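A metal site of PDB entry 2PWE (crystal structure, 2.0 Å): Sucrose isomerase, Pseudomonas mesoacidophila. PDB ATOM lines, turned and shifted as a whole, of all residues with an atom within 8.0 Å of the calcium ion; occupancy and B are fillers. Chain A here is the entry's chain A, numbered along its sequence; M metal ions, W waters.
The side-chain hydroxyl of Thr 431 lies within hydrogen-bond range of the side-chain carboxylate of Asp 21.
OD2 of Asp 21 sits close to N of Gly 24, at 3.2 Å.
OD1 of Asp 29 is in hydrogen-bond range of OG1 of Thr 22 (2.8 Å).
O of Phe 430 sits at hydrogen-bond distance from N of Asp 21 (3.0 Å).
The backbone NH (N) of Gly 26 sits at hydrogen-bond distance from the side-chain carboxylate (OD2) of Asp 21.
The backbone NH (N) of Gly 32 lies within hydrogen-bond range of the side-chain carboxylate (OD1) of Asp 29.
The backbone NH (N) of Asp 29 is in hydrogen-bond range of the backbone carbonyl oxygen (O) of Lys 20, 3.0 Å away.
Within 4 Å of the calcium ion: Asp 21, Asn 23, Asp 25, Ile 27 and Asp 29.
The nearest printed residue that does not touch the calcium ion is Thr 22 (4.2 Å).
The calcium ion is bound by the side-chain carboxylate (OD2) of Asp 29 (2.3 Å), water W1 (2.3 Å), the side-chain carboxylate (OD1) of Asp 21 (2.3 Å), the side-chain amide oxygen (OD1) of Asn 23 (2.4 Å), the backbone carbonyl oxygen (O) of Ile 27 (2.4 Å), water W2 (2.4 Å) and the side-chain carboxylate (OD1) of Asp 25 (2.5 Å).
Water W2 bridges the backbone carbonyl oxygen (O) of Glu 74 (3.1 Å) and the side-chain amide nitrogen (ND2) of Asn 23 (3.4 Å).
Water W1 bridges OD2 of Asp 25 (2.6 Å) and O of Glu 74 (2.7 Å).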
ATOM      1  N   PRO A  16      -7.142  -1.222  11.301  1.00  0.00           N
ATOM      2  CA  PRO A  16      -7.087  -1.728   9.912  1.00  0.00           C
ATOM      3  C   PRO A  16      -6.931  -0.766   8.756  1.00  0.00           C
ATOM      4  O   PRO A  16      -6.205  -1.047   7.783  1.00  0.00           O
ATOM      5  CB  PRO A  16      -8.362  -2.607   9.785  1.00  0.00           C
ATOM      6  CG  PRO A  16      -8.656  -3.022  11.206  1.00  0.00           C
ATOM      7  CD  PRO A  16      -8.351  -1.706  11.985  1.00  0.00           C
ATOM      8  N   ARG A  17      -7.597   0.373   8.857  1.00  0.00           N
ATOM      9  CA  ARG A  17      -7.559   1.362   7.791  1.00  0.00           C
ATOM     10  C   ARG A  17      -6.115   1.786   7.492  1.00  0.00           C
ATOM     11  O   ARG A  17      -5.775   2.138   6.357  1.00  0.00           O
ATOM     12  CB  ARG A  17      -8.400   2.562   8.234  1.00  0.00           C
ATOM     13  CG  ARG A  17      -8.684   3.562   7.156  1.00  0.00           C
ATOM     14  CD  ARG A  17      -9.436   4.780   7.707  1.00  0.00           C
ATOM     15  NE  ARG A  17      -9.675   5.743   6.640  1.00  0.00           N
ATOM     16  CZ  ARG A  17     -10.645   5.640   5.719  1.00  0.00           C
ATOM     17  NH1 ARG A  17     -11.497   4.614   5.732  1.00  0.00           N
ATOM     18  NH2 ARG A  17     -10.751   6.571   4.766  1.00  0.00           N
ATOM     19  N   LYS A  20      -2.359  -2.358   6.651  1.00  0.00           N
ATOM     20  CA  LYS A  20      -1.775  -2.858   5.412  1.00  0.00           C
ATOM     21  C   LYS A  20      -2.769  -2.959   4.276  1.00  0.00           C
ATOM     22  O   LYS A  20      -3.777  -3.641   4.379  1.00  0.00           O
ATOM     23  CB  LYS A  20      -1.131  -4.218   5.612  1.00  0.00           C
ATOM     24  CG  LYS A  20      -0.680  -4.858   4.317  1.00  0.00           C
ATOM     25  CD  LYS A  20       0.604  -4.252   3.754  1.00  0.00           C
ATOM     26  CE  LYS A  20       1.128  -5.134   2.586  1.00  0.00           C
ATOM     27  NZ  LYS A  20       2.452  -4.657   2.050  1.00  0.00           N
ATOM     28  N   ASP A  21      -2.496  -2.244   3.196  1.00  0.00           N
ATOM     29  CA  ASP A  21      -3.378  -2.251   2.044  1.00  0.00           C
ATOM     30  C   ASP A  21      -2.865  -3.342   1.093  1.00  0.00           C
ATOM     31  O   ASP A  21      -1.650  -3.502   0.939  1.00  0.00           O
ATOM     32  CB  ASP A  21      -3.364  -0.881   1.366  1.00  0.00           C
ATOM     33  CG  ASP A  21      -4.202  -0.827   0.104  1.00  0.00           C
ATOM     34  OD1 ASP A  21      -5.151  -1.622  -0.035  1.00  0.00           O
ATOM     35  OD2 ASP A  21      -3.918   0.033  -0.738  1.00  0.00           O
ATOM     36  N   THR A  22      -3.781  -4.091   0.488  1.00  0.00           N
ATOM     37  CA  THR A  22      -3.365  -5.140  -0.444  1.00  0.00           C
ATOM     38  C   THR A  22      -4.029  -5.036  -1.803  1.00  0.00           C
ATOM     39  O   THR A  22      -3.891  -5.953  -2.602  1.00  0.00           O
ATOM     40  CB  THR A  22      -3.653  -6.569   0.075  1.00  0.00           C
ATOM     41  OG1 THR A  22      -5.051  -6.684   0.349  1.00  0.00           O
ATOM     42  CG2 THR A  22      -2.841  -6.866   1.333  1.00  0.00           C
ATOM     43  N   ASN A  23      -4.785  -3.975  -2.066  1.00  0.00           N
ATOM     44  CA  ASN A  23      -5.409  -3.867  -3.384  1.00  0.00           C
ATOM     45  C   ASN A  23      -5.229  -2.437  -3.912  1.00  0.00           C
ATOM     46  O   ASN A  23      -6.004  -1.967  -4.770  1.00  0.00           O
ATOM     47  CB  ASN A  23      -6.893  -4.222  -3.314  1.00  0.00           C
ATOM     48  CG  ASN A  23      -7.703  -3.137  -2.661  1.00  0.00           C
ATOM     49  OD1 ASN A  23      -7.170  -2.374  -1.853  1.00  0.00           O
ATOM     50  ND2 ASN A  23      -8.972  -3.056  -2.996  1.00  0.00           N
ATOM     51  N   GLY A  24      -4.227  -1.751  -3.366  1.00  0.00           N
ATOM     52  CA  GLY A  24      -3.899  -0.395  -3.789  1.00  0.00           C
ATOM     53  C   GLY A  24      -4.927   0.726  -3.809  1.00  0.00           C
ATOM     54  O   GLY A  24      -4.769   1.700  -4.565  1.00  0.00           O
ATOM     55  N   ASP A  25      -5.984   0.622  -3.020  1.00  0.00           N
ATOM     56  CA  ASP A  25      -6.953   1.706  -3.029  1.00  0.00           C
ATOM     57  C   ASP A  25      -6.522   2.706  -1.974  1.00  0.00           C
ATOM     58  O   ASP A  25      -7.193   3.702  -1.738  1.00  0.00           O
ATOM     59  CB  ASP A  25      -8.376   1.203  -2.745  1.00  0.00           C
ATOM     60  CG  ASP A  25      -8.511   0.521  -1.382  1.00  0.00           C
ATOM     61  OD1 ASP A  25      -7.510   0.386  -0.645  1.00  0.00           O
ATOM     62  OD2 ASP A  25      -9.655   0.126  -1.072  1.00  0.00           O
ATOM     63  N   GLY A  26      -5.408   2.422  -1.315  1.00  0.00           N
ATOM     64  CA  GLY A  26      -4.938   3.344  -0.298  1.00  0.00           C
ATOM     65  C   GLY A  26      -5.492   3.131   1.109  1.00  0.00           C
ATOM     66  O   GLY A  26      -5.160   3.886   2.024  1.00  0.00           O
ATOM     67  N   ILE A  27      -6.355   2.131   1.277  1.00  0.00           N
ATOM     68  CA  ILE A  27      -6.924   1.866   2.608  1.00  0.00           C
ATOM     69  C   ILE A  27      -6.552   0.446   3.044  1.00  0.00           C
ATOM     70  O   ILE A  27      -6.604  -0.493   2.257  1.00  0.00           O
ATOM     71  CB  ILE A  27      -8.444   2.026   2.578  1.00  0.00           C
ATOM     72  CG1 ILE A  27      -8.780   3.507   2.461  1.00  0.00           C
ATOM     73  CG2 ILE A  27      -9.084   1.379   3.817  1.00  0.00           C
ATOM     74  CD1 ILE A  27     -10.154   3.753   1.771  1.00  0.00           C
ATOM     75  N   GLY A  28      -6.119   0.295   4.300  1.00  0.00           N
ATOM     76  CA  GLY A  28      -5.729  -1.038   4.782  1.00  0.00           C
ATOM     77  C   GLY A  28      -6.946  -1.959   4.783  1.00  0.00           C
ATOM     78  O   GLY A  28      -8.063  -1.491   4.874  1.00  0.00           O
ATOM     79  N   ASP A  29      -6.735  -3.266   4.739  1.00  0.00           N
ATOM     80  CA  ASP A  29      -7.844  -4.214   4.683  1.00  0.00           C
ATOM     81  C   ASP A  29      -7.513  -5.510   5.408  1.00  0.00           C
ATOM     82  O   ASP A  29      -6.396  -5.686   5.906  1.00  0.00           O
ATOM     83  CB  ASP A  29      -8.155  -4.504   3.222  1.00  0.00           C
ATOM     84  CG  ASP A  29      -6.902  -4.634   2.386  1.00  0.00           C
ATOM     85  OD1 ASP A  29      -6.099  -5.561   2.636  1.00  0.00           O
ATOM     86  OD2 ASP A  29      -6.687  -3.792   1.500  1.00  0.00           O
ATOM     87  N   PHE A  30      -8.494  -6.410   5.480  1.00  0.00           N
ATOM     88  CA  PHE A  30      -8.345  -7.691   6.166  1.00  0.00           C
ATOM     89  C   PHE A  30      -7.253  -8.568   5.560  1.00  0.00           C
ATOM     90  O   PHE A  30      -6.492  -9.197   6.285  1.00  0.00           O
ATOM     91  CB  PHE A  30      -9.647  -8.502   6.116  1.00  0.00           C
ATOM     92  CG  PHE A  30     -10.732  -7.994   7.009  1.00  0.00           C
ATOM     93  CD1 PHE A  30     -10.473  -7.682   8.333  1.00  0.00           C
ATOM     94  CD2 PHE A  30     -12.050  -7.942   6.547  1.00  0.00           C
ATOM     95  CE1 PHE A  30     -11.497  -7.305   9.184  1.00  0.00           C
ATOM     96  CE2 PHE A  30     -13.098  -7.564   7.380  1.00  0.00           C
ATOM     97  CZ  PHE A  30     -12.831  -7.249   8.715  1.00  0.00           C
ATOM     98  N   LYS A  31      -7.201  -8.635   4.242  1.00  0.00           N
ATOM     99  CA  LYS A  31      -6.179  -9.466   3.588  1.00  0.00           C
ATOM    100  C   LYS A  31      -4.804  -8.962   4.023  1.00  0.00           C
ATOM    101  O   LYS A  31      -3.872  -9.746   4.288  1.00  0.00           O
ATOM    102  CB  LYS A  31      -6.344  -9.390   2.050  1.00  0.00           C
ATOM    103  N   GLY A  32      -4.679  -7.636   4.136  1.00  0.00           N
ATOM    104  CA  GLY A  32      -3.399  -7.081   4.549  1.00  0.00           C
ATOM    105  C   GLY A  32      -3.059  -7.487   5.979  1.00  0.00           C
ATOM    106  O   GLY A  32      -1.936  -7.835   6.269  1.00  0.00           O
ATOM    107  N   LYS A  73     -16.997  -2.740   3.544  1.00  0.00           N
ATOM    108  CA  LYS A  73     -16.611  -2.998   2.137  1.00  0.00           C
ATOM    109  C   LYS A  73     -15.098  -2.788   1.935  1.00  0.00           C
ATOM    110  O   LYS A  73     -14.427  -3.625   1.329  1.00  0.00           O
ATOM    111  CB  LYS A  73     -17.414  -2.070   1.186  1.00  0.00           C
ATOM    112  N   GLU A  74     -14.579  -1.691   2.452  1.00  0.00           N
ATOM    113  CA  GLU A  74     -13.157  -1.402   2.327  1.00  0.00           C
ATOM    114  C   GLU A  74     -12.242  -2.474   2.940  1.00  0.00           C
ATOM    115  O   GLU A  74     -11.110  -2.634   2.488  1.00  0.00           O
ATOM    116  CB  GLU A  74     -12.815  -0.062   2.992  1.00  0.00           C
ATOM    117  CG  GLU A  74     -13.257   1.183   2.236  1.00  0.00           C
ATOM    118  CD  GLU A  74     -14.738   1.462   2.373  1.00  0.00           C
ATOM    119  OE1 GLU A  74     -15.415   0.741   3.146  1.00  0.00           O
ATOM    120  OE2 GLU A  74     -15.230   2.396   1.718  1.00  0.00           O
ATOM    121  N   TYR A  75     -12.690  -3.180   3.978  1.00  0.00           N
ATOM    122  CA  TYR A  75     -11.803  -4.163   4.600  1.00  0.00           C
ATOM    123  C   TYR A  75     -11.857  -5.542   3.962  1.00  0.00           C
ATOM    124  O   TYR A  75     -10.918  -6.327   4.104  1.00  0.00           O
ATOM    125  CB  TYR A  75     -12.046  -4.250   6.114  1.00  0.00           C
ATOM    126  CG  TYR A  75     -11.757  -2.956   6.875  1.00  0.00           C
ATOM    127  CD1 TYR A  75     -11.086  -1.882   6.267  1.00  0.00           C
ATOM    128  CD2 TYR A  75     -12.186  -2.780   8.207  1.00  0.00           C
ATOM    129  CE1 TYR A  75     -10.862  -0.673   6.944  1.00  0.00           C
ATOM    130  CE2 TYR A  75     -11.969  -1.581   8.890  1.00  0.00           C
ATOM    131  CZ  TYR A  75     -11.316  -0.521   8.246  1.00  0.00           C
ATOM    132  OH  TYR A  75     -11.237   0.720   8.843  1.00  0.00           O
ATOM    133  N   GLY A  76     -12.958  -5.827   3.262  1.00  0.00           N
ATOM    134  CA  GLY A  76     -13.103  -7.107   2.579  1.00  0.00           C
ATOM    135  C   GLY A  76     -14.510  -7.677   2.623  1.00  0.00           C
ATOM    136  O   GLY A  76     -15.507  -6.935   2.534  1.00  0.00           O
ATOM    137  N   PHE A 430       3.121   0.351   2.684  1.00  0.00           N
ATOM    138  CA  PHE A 430       1.764   0.253   3.148  1.00  0.00           C
ATOM    139  C   PHE A 430       0.770   0.049   2.000  1.00  0.00           C
ATOM    140  O   PHE A 430      -0.255  -0.612   2.147  1.00  0.00           O
ATOM    141  CB  PHE A 430       1.396   1.518   3.949  1.00  0.00           C
ATOM    142  CG  PHE A 430      -0.063   1.743   4.083  1.00  0.00           C
ATOM    143  CD1 PHE A 430      -0.862   0.873   4.837  1.00  0.00           C
ATOM    144  CD2 PHE A 430      -0.670   2.821   3.426  1.00  0.00           C
ATOM    145  CE1 PHE A 430      -2.225   1.061   4.943  1.00  0.00           C
ATOM    146  CE2 PHE A 430      -2.041   3.036   3.523  1.00  0.00           C
ATOM    147  CZ  PHE A 430      -2.839   2.145   4.291  1.00  0.00           C
ATOM    148  N   THR A 431       1.078   0.613   0.839  1.00  0.00           N
ATOM    149  CA  THR A 431       0.168   0.512  -0.307  1.00  0.00           C
ATOM    150  C   THR A 431       0.917   0.722  -1.617  1.00  0.00           C
ATOM    151  O   THR A 431       2.022   1.280  -1.622  1.00  0.00           O
ATOM    152  CB  THR A 431      -0.927   1.587  -0.229  1.00  0.00           C
ATOM    153  OG1 THR A 431      -1.740   1.524  -1.402  1.00  0.00           O
ATOM    154  CG2 THR A 431      -0.322   2.993  -0.136  1.00  0.00           C
HETATM  155 CA    CA M   1      -7.365  -1.901   0.448  1.00  0.00          CA
HETATM  156  O   HOH W   1      -9.334  -1.061   1.226  1.00  0.00           O
HETATM  157  O   HOH W   2      -9.145  -3.566   0.333  1.00  0.00           O
